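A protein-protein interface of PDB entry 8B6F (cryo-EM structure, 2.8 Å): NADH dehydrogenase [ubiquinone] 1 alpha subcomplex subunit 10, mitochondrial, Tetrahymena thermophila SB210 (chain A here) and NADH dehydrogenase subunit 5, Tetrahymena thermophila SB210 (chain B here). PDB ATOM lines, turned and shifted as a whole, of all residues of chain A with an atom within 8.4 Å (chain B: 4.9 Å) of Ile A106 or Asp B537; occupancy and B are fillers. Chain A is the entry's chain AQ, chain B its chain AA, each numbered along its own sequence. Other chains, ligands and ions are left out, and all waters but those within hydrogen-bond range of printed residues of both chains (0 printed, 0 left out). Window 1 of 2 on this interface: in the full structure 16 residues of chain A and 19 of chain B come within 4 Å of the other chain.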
ATOM      1  N   ALA A   4      17.359  26.912  19.613  1.00  0.00           N
ATOM      2  CA  ALA A   4      17.279  25.641  20.333  1.00  0.00           C
ATOM      3  C   ALA A   4      18.309  24.644  19.815  1.00  0.00           C
ATOM      4  O   ALA A   4      18.026  23.457  19.647  1.00  0.00           O
ATOM      5  CB  ALA A   4      15.872  25.052  20.241  1.00  0.00           C
ATOM      6  N   TYR A   6      21.313  24.093  21.412  1.00  0.00           N
ATOM      7  CA  TYR A   6      22.291  24.024  22.492  1.00  0.00           C
ATOM      8  C   TYR A   6      23.121  22.752  22.413  1.00  0.00           C
ATOM      9  O   TYR A   6      24.347  22.789  22.569  1.00  0.00           O
ATOM     10  CB  TYR A   6      21.598  24.107  23.850  1.00  0.00           C
ATOM     11  CG  TYR A   6      20.538  25.172  23.972  1.00  0.00           C
ATOM     12  CD1 TYR A   6      20.894  26.502  24.114  1.00  0.00           C
ATOM     13  CD2 TYR A   6      19.186  24.849  23.979  1.00  0.00           C
ATOM     14  CE1 TYR A   6      19.944  27.484  24.241  1.00  0.00           C
ATOM     15  CE2 TYR A   6      18.221  25.833  24.109  1.00  0.00           C
ATOM     16  CZ  TYR A   6      18.615  27.150  24.249  1.00  0.00           C
ATOM     17  OH  TYR A   6      17.695  28.163  24.379  1.00  0.00           O
ATOM     18  N   PHE A   7      22.475  21.620  22.166  1.00  0.00           N
ATOM     19  CA  PHE A   7      23.124  20.320  22.203  1.00  0.00           C
ATOM     20  C   PHE A   7      23.719  19.924  20.862  1.00  0.00           C
ATOM     21  O   PHE A   7      24.191  18.794  20.713  1.00  0.00           O
ATOM     22  CB  PHE A   7      22.123  19.263  22.671  1.00  0.00           C
ATOM     23  CG  PHE A   7      21.368  19.662  23.907  1.00  0.00           C
ATOM     24  CD1 PHE A   7      21.999  20.355  24.926  1.00  0.00           C
ATOM     25  CD2 PHE A   7      20.024  19.363  24.038  1.00  0.00           C
ATOM     26  CE1 PHE A   7      21.310  20.730  26.057  1.00  0.00           C
ATOM     27  CE2 PHE A   7      19.328  19.736  25.168  1.00  0.00           C
ATOM     28  CZ  PHE A   7      19.972  20.419  26.179  1.00  0.00           C
ATOM     29  N   ARG A  45      11.379  31.147  32.953  1.00  0.00           N
ATOM     30  CA  ARG A  45      11.096  29.994  32.108  1.00  0.00           C
ATOM     31  C   ARG A  45      11.539  28.703  32.784  1.00  0.00           C
ATOM     32  O   ARG A  45      10.806  27.707  32.785  1.00  0.00           O
ATOM     33  CB  ARG A  45      11.795  30.162  30.759  1.00  0.00           C
ATOM     34  CG  ARG A  45      11.501  29.055  29.764  1.00  0.00           C
ATOM     35  CD  ARG A  45      12.327  29.217  28.499  1.00  0.00           C
ATOM     36  NE  ARG A  45      12.076  30.491  27.838  1.00  0.00           N
ATOM     37  CZ  ARG A  45      11.078  30.716  26.995  1.00  0.00           C
ATOM     38  NH1 ARG A  45      10.201  29.773  26.695  1.00  0.00           N
ATOM     39  NH2 ARG A  45      10.958  31.917  26.438  1.00  0.00           N
ATOM     40  N   ARG A  46      12.743  28.695  33.360  1.00  0.00           N
ATOM     41  CA  ARG A  46      13.244  27.482  33.996  1.00  0.00           C
ATOM     42  C   ARG A  46      12.451  27.143  35.253  1.00  0.00           C
ATOM     43  O   ARG A  46      12.169  25.968  35.516  1.00  0.00           O
ATOM     44  CB  ARG A  46      14.727  27.641  34.320  1.00  0.00           C
ATOM     45  CG  ARG A  46      15.400  26.366  34.800  1.00  0.00           C
ATOM     46  CD  ARG A  46      15.389  25.264  33.751  1.00  0.00           C
ATOM     47  NE  ARG A  46      15.918  25.714  32.468  1.00  0.00           N
ATOM     48  CZ  ARG A  46      15.218  25.823  31.346  1.00  0.00           C
ATOM     49  NH1 ARG A  46      13.939  25.488  31.286  1.00  0.00           N
ATOM     50  NH2 ARG A  46      15.818  26.276  30.250  1.00  0.00           N
ATOM     51  N   ALA A  49       9.325  25.613  34.175  1.00  0.00           N
ATOM     52  CA  ALA A  49       9.533  24.262  33.670  1.00  0.00           C
ATOM     53  C   ALA A  49       9.691  23.258  34.805  1.00  0.00           C
ATOM     54  O   ALA A  49       9.249  22.110  34.687  1.00  0.00           O
ATOM     55  CB  ALA A  49      10.758  24.231  32.758  1.00  0.00           C
ATOM     56  N   HIS A  50      10.324  23.660  35.907  1.00  0.00           N
ATOM     57  CA  HIS A  50      10.634  22.725  36.981  1.00  0.00           C
ATOM     58  C   HIS A  50       9.595  22.693  38.093  1.00  0.00           C
ATOM     59  O   HIS A  50       9.494  21.676  38.787  1.00  0.00           O
ATOM     60  CB  HIS A  50      11.997  23.057  37.593  1.00  0.00           C
ATOM     61  CG  HIS A  50      13.151  22.500  36.823  1.00  0.00           C
ATOM     62  ND1 HIS A  50      13.494  22.953  35.567  1.00  0.00           N
ATOM     63  CD2 HIS A  50      14.034  21.521  37.124  1.00  0.00           C
ATOM     64  CE1 HIS A  50      14.542  22.279  35.130  1.00  0.00           C
ATOM     65  NE2 HIS A  50      14.890  21.404  36.057  1.00  0.00           N
ATOM     66  N   GLU A  53       5.382  22.669  35.300  1.00  0.00           N
ATOM     67  CA  GLU A  53       5.375  21.479  34.452  1.00  0.00           C
ATOM     68  C   GLU A  53       6.507  20.544  34.875  1.00  0.00           C
ATOM     69  O   GLU A  53       7.502  20.357  34.176  1.00  0.00           O
ATOM     70  CB  GLU A  53       5.492  21.877  32.983  1.00  0.00           C
ATOM     71  CG  GLU A  53       4.368  22.779  32.507  1.00  0.00           C
ATOM     72  CD  GLU A  53       4.465  23.099  31.026  1.00  0.00           C
ATOM     73  OE1 GLU A  53       5.539  22.865  30.436  1.00  0.00           O
ATOM     74  OE2 GLU A  53       3.464  23.581  30.453  1.00  0.00           O
ATOM     75  N   GLY A  54       6.331  19.948  36.051  1.00  0.00           N
ATOM     76  CA  GLY A  54       7.334  19.061  36.606  1.00  0.00           C
ATOM     77  C   GLY A  54       6.745  17.834  37.270  1.00  0.00           C
ATOM     78  O   GLY A  54       5.637  17.409  36.934  1.00  0.00           O
ATOM     79  N   TYR A  55       7.481  17.255  38.216  1.00  0.00           N
ATOM     80  CA  TYR A  55       7.049  16.063  38.938  1.00  0.00           C
ATOM     81  C   TYR A  55       6.427  16.503  40.258  1.00  0.00           C
ATOM     82  O   TYR A  55       7.121  17.039  41.128  1.00  0.00           O
ATOM     83  CB  TYR A  55       8.223  15.118  39.181  1.00  0.00           C
ATOM     84  CG  TYR A  55       9.240  15.090  38.066  1.00  0.00           C
ATOM     85  CD1 TYR A  55       9.052  14.292  36.945  1.00  0.00           C
ATOM     86  CD2 TYR A  55      10.397  15.852  38.142  1.00  0.00           C
ATOM     87  CE1 TYR A  55       9.984  14.261  35.926  1.00  0.00           C
ATOM     88  CE2 TYR A  55      11.334  15.830  37.128  1.00  0.00           C
ATOM     89  CZ  TYR A  55      11.123  15.032  36.024  1.00  0.00           C
ATOM     90  OH  TYR A  55      12.057  15.007  35.015  1.00  0.00           O
ATOM     91  N   ASP A 102      18.649  20.695  32.660  1.00  0.00           N
ATOM     92  CA  ASP A 102      18.124  19.340  32.516  1.00  0.00           C
ATOM     93  C   ASP A 102      18.452  18.819  31.126  1.00  0.00           C
ATOM     94  O   ASP A 102      17.889  19.323  30.133  1.00  0.00           O
ATOM     95  CB  ASP A 102      16.617  19.325  32.750  1.00  0.00           C
ATOM     96  CG  ASP A 102      16.033  17.929  32.699  1.00  0.00           C
ATOM     97  OD1 ASP A 102      16.810  16.959  32.583  1.00  0.00           O
ATOM     98  OD2 ASP A 102      14.793  17.802  32.774  1.00  0.00           O
ATOM     99  N   PRO A 103      19.337  17.833  30.991  1.00  0.00           N
ATOM    100  CA  PRO A 103      19.499  17.188  29.687  1.00  0.00           C
ATOM    101  C   PRO A 103      18.176  16.598  29.227  1.00  0.00           C
ATOM    102  O   PRO A 103      17.389  16.091  30.028  1.00  0.00           O
ATOM    103  CB  PRO A 103      20.549  16.103  29.952  1.00  0.00           C
ATOM    104  CG  PRO A 103      21.302  16.585  31.134  1.00  0.00           C
ATOM    105  CD  PRO A 103      20.306  17.328  31.978  1.00  0.00           C
ATOM    106  N   ALA A 104      17.926  16.685  27.924  1.00  0.00           N
ATOM    107  CA  ALA A 104      16.661  16.247  27.342  1.00  0.00           C
ATOM    108  C   ALA A 104      15.490  17.083  27.854  1.00  0.00           C
ATOM    109  O   ALA A 104      14.368  16.587  27.981  1.00  0.00           O
ATOM    110  CB  ALA A 104      16.409  14.760  27.612  1.00  0.00           C
ATOM    111  N   MET A 105      15.742  18.351  28.161  1.00  0.00           N
ATOM    112  CA  MET A 105      14.667  19.252  28.545  1.00  0.00           C
ATOM    113  C   MET A 105      13.720  19.473  27.371  1.00  0.00           C
ATOM    114  O   MET A 105      14.113  19.398  26.205  1.00  0.00           O
ATOM    115  CB  MET A 105      15.227  20.591  29.019  1.00  0.00           C
ATOM    116  CG  MET A 105      16.092  21.299  27.990  1.00  0.00           C
ATOM    117  SD  MET A 105      16.660  22.908  28.564  1.00  0.00           S
ATOM    118  CE  MET A 105      17.609  23.448  27.150  1.00  0.00           C
ATOM    119  N   ILE A 106      12.456  19.750  27.692  1.00  0.00           N
ATOM    120  CA  ILE A 106      11.446  19.893  26.653  1.00  0.00           C
ATOM    121  C   ILE A 106      11.782  21.090  25.779  1.00  0.00           C
ATOM    122  O   ILE A 106      11.995  22.204  26.273  1.00  0.00           O
ATOM    123  CB  ILE A 106      10.049  20.026  27.277  1.00  0.00           C
ATOM    124  CG1 ILE A 106       9.714  18.774  28.090  1.00  0.00           C
ATOM    125  CG2 ILE A 106       9.005  20.251  26.190  1.00  0.00           C
ATOM    126  CD1 ILE A 106       8.420  18.868  28.869  1.00  0.00           C
ATOM    127  N   ILE A 107      11.831  20.863  24.470  1.00  0.00           N
ATOM    128  CA  ILE A 107      12.050  21.914  23.484  1.00  0.00           C
ATOM    129  C   ILE A 107      10.767  22.050  22.679  1.00  0.00           C
ATOM    130  O   ILE A 107      10.298  21.075  22.079  1.00  0.00           O
ATOM    131  CB  ILE A 107      13.248  21.603  22.576  1.00  0.00           C
ATOM    132  CG1 ILE A 107      14.527  21.496  23.413  1.00  0.00           C
ATOM    133  CG2 ILE A 107      13.397  22.675  21.499  1.00  0.00           C
ATOM    134  CD1 ILE A 107      15.743  21.037  22.635  1.00  0.00           C
ATOM    135  N   ASP A 108      10.200  23.252  22.664  1.00  0.00           N
ATOM    136  CA  ASP A 108       8.937  23.462  21.974  1.00  0.00           C
ATOM    137  C   ASP A 108       9.099  23.196  20.483  1.00  0.00           C
ATOM    138  O   ASP A 108      10.146  23.474  19.895  1.00  0.00           O
ATOM    139  CB  ASP A 108       8.441  24.886  22.209  1.00  0.00           C
ATOM    140  CG  ASP A 108       6.975  25.053  21.876  1.00  0.00           C
ATOM    141  OD1 ASP A 108       6.521  24.468  20.873  1.00  0.00           O
ATOM    142  OD2 ASP A 108       6.274  25.764  22.626  1.00  0.00           O
ATOM    143  N   GLU A 109       8.050  22.645  19.871  1.00  0.00           N
ATOM    144  CA  GLU A 109       8.109  22.300  18.457  1.00  0.00           C
ATOM    145  C   GLU A 109       8.113  23.521  17.549  1.00  0.00           C
ATOM    146  O   GLU A 109       8.369  23.377  16.350  1.00  0.00           O
ATOM    147  CB  GLU A 109       6.926  21.403  18.089  1.00  0.00           C
ATOM    148  CG  GLU A 109       6.697  20.220  19.028  1.00  0.00           C
ATOM    149  CD  GLU A 109       7.819  19.197  18.993  1.00  0.00           C
ATOM    150  OE1 GLU A 109       9.000  19.592  18.918  1.00  0.00           O
ATOM    151  OE2 GLU A 109       7.518  17.987  19.041  1.00  0.00           O
ATOM    152  N   ARG A 111      10.224  25.974  17.684  1.00  0.00           N
ATOM    153  CA  ARG A 111      11.559  26.536  17.604  1.00  0.00           C
ATOM    154  C   ARG A 111      12.412  25.775  16.596  1.00  0.00           C
ATOM    155  O   ARG A 111      12.205  24.578  16.378  1.00  0.00           O
ATOM    156  CB  ARG A 111      12.226  26.484  18.978  1.00  0.00           C
ATOM    157  CG  ARG A 111      11.483  27.269  20.042  1.00  0.00           C
ATOM    158  CD  ARG A 111      12.056  26.979  21.403  1.00  0.00           C
ATOM    159  NE  ARG A 111      13.464  27.336  21.459  1.00  0.00           N
ATOM    160  CZ  ARG A 111      14.238  27.172  22.521  1.00  0.00           C
ATOM    161  NH1 ARG A 111      13.771  26.655  23.645  1.00  0.00           N
ATOM    162  NH2 ARG A 111      15.519  27.508  22.440  1.00  0.00           N
ATOM    163  N   ALA A 114      14.400  21.888  16.683  1.00  0.00           N
ATOM    164  CA  ALA A 114      13.660  21.043  17.602  1.00  0.00           C
ATOM    165  C   ALA A 114      13.265  19.740  16.919  1.00  0.00           C
ATOM    166  O   ALA A 114      13.325  19.606  15.695  1.00  0.00           O
ATOM    167  CB  ALA A 114      12.416  21.764  18.114  1.00  0.00           C
ATOM    168  N   SER B 478      11.766  10.619  32.254  1.00  0.00           N
ATOM    169  CA  SER B 478      10.619  11.513  32.177  1.00  0.00           C
ATOM    170  C   SER B 478       9.887  11.456  30.845  1.00  0.00           C
ATOM    171  O   SER B 478       8.758  11.953  30.762  1.00  0.00           O
ATOM    172  CB  SER B 478      11.049  12.966  32.440  1.00  0.00           C
ATOM    173  OG  SER B 478      11.905  13.441  31.417  1.00  0.00           O
ATOM    174  N   ASP B 479      10.485  10.877  29.811  1.00  0.00           N
ATOM    175  CA  ASP B 479       9.865  10.763  28.500  1.00  0.00           C
ATOM    176  C   ASP B 479       9.278   9.368  28.328  1.00  0.00           C
ATOM    177  O   ASP B 479       9.850   8.380  28.797  1.00  0.00           O
ATOM    178  CB  ASP B 479      10.891  11.046  27.401  1.00  0.00           C
ATOM    179  CG  ASP B 479      10.284  11.028  26.017  1.00  0.00           C
ATOM    180  OD1 ASP B 479       9.076  10.743  25.904  1.00  0.00           O
ATOM    181  OD2 ASP B 479      11.013  11.297  25.041  1.00  0.00           O
ATOM    182  N   ASN B 532      -1.054  14.724  22.467  1.00  0.00           N
ATOM    183  CA  ASN B 532      -0.273  15.805  23.052  1.00  0.00           C
ATOM    184  C   ASN B 532       0.581  16.541  22.024  1.00  0.00           C
ATOM    185  O   ASN B 532       1.407  17.373  22.409  1.00  0.00           O
ATOM    186  CB  ASN B 532       0.615  15.260  24.173  1.00  0.00           C
ATOM    187  CG  ASN B 532       1.210  16.357  25.029  1.00  0.00           C
ATOM    188  OD1 ASN B 532       0.723  17.485  25.035  1.00  0.00           O
ATOM    189  ND2 ASN B 532       2.272  16.032  25.755  1.00  0.00           N
ATOM    190  N   ILE B 535       4.655  15.888  21.752  1.00  0.00           N
ATOM    191  CA  ILE B 535       5.419  16.135  22.970  1.00  0.00           C
ATOM    192  C   ILE B 535       5.383  14.852  23.790  1.00  0.00           C
ATOM    193  O   ILE B 535       4.352  14.505  24.371  1.00  0.00           O
ATOM    194  CB  ILE B 535       4.861  17.326  23.760  1.00  0.00           C
ATOM    195  CG1 ILE B 535       5.037  18.627  22.972  1.00  0.00           C
ATOM    196  CG2 ILE B 535       5.531  17.428  25.130  1.00  0.00           C
ATOM    197  CD1 ILE B 535       6.480  19.068  22.784  1.00  0.00           C
ATOM    198  N   GLN B 536       6.509  14.147  23.832  1.00  0.00           N
ATOM    199  CA  GLN B 536       6.581  12.832  24.453  1.00  0.00           C
ATOM    200  C   GLN B 536       6.866  12.887  25.946  1.00  0.00           C
ATOM    201  O   GLN B 536       6.810  11.847  26.609  1.00  0.00           O
ATOM    202  CB  GLN B 536       7.660  11.990  23.769  1.00  0.00           C
ATOM    203  CG  GLN B 536       7.574  11.981  22.255  1.00  0.00           C
ATOM    204  CD  GLN B 536       8.728  11.239  21.626  1.00  0.00           C
ATOM    205  OE1 GLN B 536       9.589  10.704  22.323  1.00  0.00           O
ATOM    206  NE2 GLN B 536       8.757  11.202  20.300  1.00  0.00           N
ATOM    207  N   ASP B 537       7.172  14.060  26.491  1.00  0.00           N
ATOM    208  CA  ASP B 537       7.475  14.202  27.907  1.00  0.00           C
ATOM    209  C   ASP B 537       6.182  14.404  28.683  1.00  0.00           C
ATOM    210  O   ASP B 537       5.359  15.246  28.312  1.00  0.00           O
ATOM    211  CB  ASP B 537       8.418  15.383  28.131  1.00  0.00           C
ATOM    212  CG  ASP B 537       8.980  15.424  29.533  1.00  0.00           C
ATOM    213  OD1 ASP B 537       8.225  15.148  30.489  1.00  0.00           O
ATOM    214  OD2 ASP B 537      10.181  15.728  29.680  1.00  0.00           O
ATOM    215  N   PHE B 538       6.005  13.638  29.761  1.00  0.00           N
ATOM    216  CA  PHE B 538       4.782  13.748  30.545  1.00  0.00           C
ATOM    217  C   PHE B 538       4.829  14.886  31.554  1.00  0.00           C
ATOM    218  O   PHE B 538       3.857  15.077  32.289  1.00  0.00           O
ATOM    219  CB  PHE B 538       4.455  12.424  31.253  1.00  0.00           C
ATOM    220  CG  PHE B 538       5.541  11.910  32.154  1.00  0.00           C
ATOM    221  CD1 PHE B 538       5.874  12.576  33.322  1.00  0.00           C
ATOM    222  CD2 PHE B 538       6.184  10.720  31.863  1.00  0.00           C
ATOM    223  CE1 PHE B 538       6.856  12.086  34.160  1.00  0.00           C
ATOM    224  CE2 PHE B 538       7.166  10.224  32.696  1.00  0.00           C
ATOM    225  CZ  PHE B 538       7.502  10.909  33.847  1.00  0.00           C
ATOM    226  N   LYS B 539       5.925  15.643  31.611  1.00  0.00           N
ATOM    227  CA  LYS B 539       5.915  16.881  32.377  1.00  0.00           C
ATOM    228  C   LYS B 539       4.938  17.892  31.794  1.00  0.00           C
ATOM    229  O   LYS B 539       4.500  18.799  32.509  1.00  0.00           O
ATOM    230  CB  LYS B 539       7.321  17.476  32.432  1.00  0.00           C
ATOM    231  CG  LYS B 539       8.280  16.683  33.305  1.00  0.00           C
ATOM    232  CD  LYS B 539       9.625  17.377  33.433  1.00  0.00           C
ATOM    233  CE  LYS B 539      10.420  17.298  32.142  1.00  0.00           C
ATOM    234  NZ  LYS B 539      11.717  18.022  32.244  1.00  0.00           N
ATOM    235  N   ARG B 540       4.593  17.760  30.514  1.00  0.00           N
ATOM    236  CA  ARG B 540       3.542  18.547  29.884  1.00  0.00           C
ATOM    237  C   ARG B 540       2.256  17.753  29.696  1.00  0.00           C
ATOM    238  O   ARG B 540       1.383  18.181  28.935  1.00  0.00           O
ATOM    239  CB  ARG B 540       4.018  19.083  28.534  1.00  0.00           C
ATOM    240  CG  ARG B 540       4.987  20.243  28.637  1.00  0.00           C
ATOM    241  CD  ARG B 540       5.331  20.786  27.262  1.00  0.00           C
ATOM    242  NE  ARG B 540       6.184  21.964  27.337  1.00  0.00           N
ATOM    243  CZ  ARG B 540       6.618  22.642  26.283  1.00  0.00           C
ATOM    244  NH1 ARG B 540       6.298  22.284  25.050  1.00  0.00           N
ATOM    245  NH2 ARG B 540       7.396  23.705  26.471  1.00  0.00           N
ATOM    246  N   MET B 541       2.125  16.607  30.355  1.00  0.00           N
ATOM    247  CA  MET B 541       0.924  15.786  30.292  1.00  0.00           C
ATOM    248  C   MET B 541       0.270  15.752  31.665  1.00  0.00           C
ATOM    249  O   MET B 541       0.949  15.551  32.675  1.00  0.00           O
ATOM    250  CB  MET B 541       1.251  14.363  29.836  1.00  0.00           C
ATOM    251  CG  MET B 541       1.877  14.272  28.457  1.00  0.00           C
ATOM    252  SD  MET B 541       2.415  12.592  28.093  1.00  0.00           S
ATOM    253  CE  MET B 541       3.251  12.829  26.531  1.00  0.00           C
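The side-chain carboxylate of Asp B537 is in salt-bridge range of the side-chain amino group of Lys B539.
O of Ser B478 sits close to N of Phe B538, at 3.4 Å.
The side-chain carboxylate (OD2) of Asp B537 sits at hydrogen-bond distance from the side-chain hydroxyl (OG) of Ser B478.
The backbone carbonyl oxygen (O) of Ile B535 is in hydrogen-bond range of the side-chain amide nitrogen (ND2) of Asn B532 (2.9 Å).
Of the printed residues of chain B, Ile A106 touches Asp B537 (3.5 Å), Lys B539 (3.98 Å) and Arg B540 (3.4 Å).
Of chain A, only Ile A106 comes within 4 Å of Asp B537.
Printed residues of chain A within 4 Å of Arg B540: Glu A53 (3.2 Å) and Ile A106 (3.4 Å).
Of the printed residues of chain B, Glu A109 touches Ile B535.
Of the printed residues of chain A, Ile B535 touches Glu A109.
Printed residues of chain B within 4 Å of Asp A102: Lys B539 (3.1 Å).
Of the printed residues of chain B, Glu A53 touches Lys B539 and Arg B540.
Arg A111 touches none of the printed residues of chain B.
Ile A107 touches none of the printed residues of chain B.
The nearest printed residue of chain B that does not touch Ile A106 is Ile B535 (4.4 Å).
The nearest printed residue of chain B that does not touch Asp A102 is Ser B478 (5.4 Å).
The side-chain amino group (NZ) of Lys B539 lies within salt-bridge range of the side-chain carboxylate (OD2) of Asp A102 (3.1 Å).
NE of Arg B540 is in salt-bridge range of OE1 of Glu A53, 3.3 Å away.
Among the printed residues, merely in contact across the chains: Glu A53 with Lys B539, Tyr A55 with Ser B478, Tyr A55 with Lys B539, Ile A106 with Asp B537, Ile A106 with Lys B539, Ile A106 with Arg B540 and Glu A109 with Ile B535.
Hydrophobic or aromatic side chains of chain A that line the printed part of chain B: Tyr A55 and Ile A106.
Among the printed residues, Asp or Glu carboxylates within 4 Å of a Lys or Arg side-chain nitrogen of the other chain: Glu A53 with Arg B540 (3.3 Å) and Asp A102 with Lys B539 (3.1 Å).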
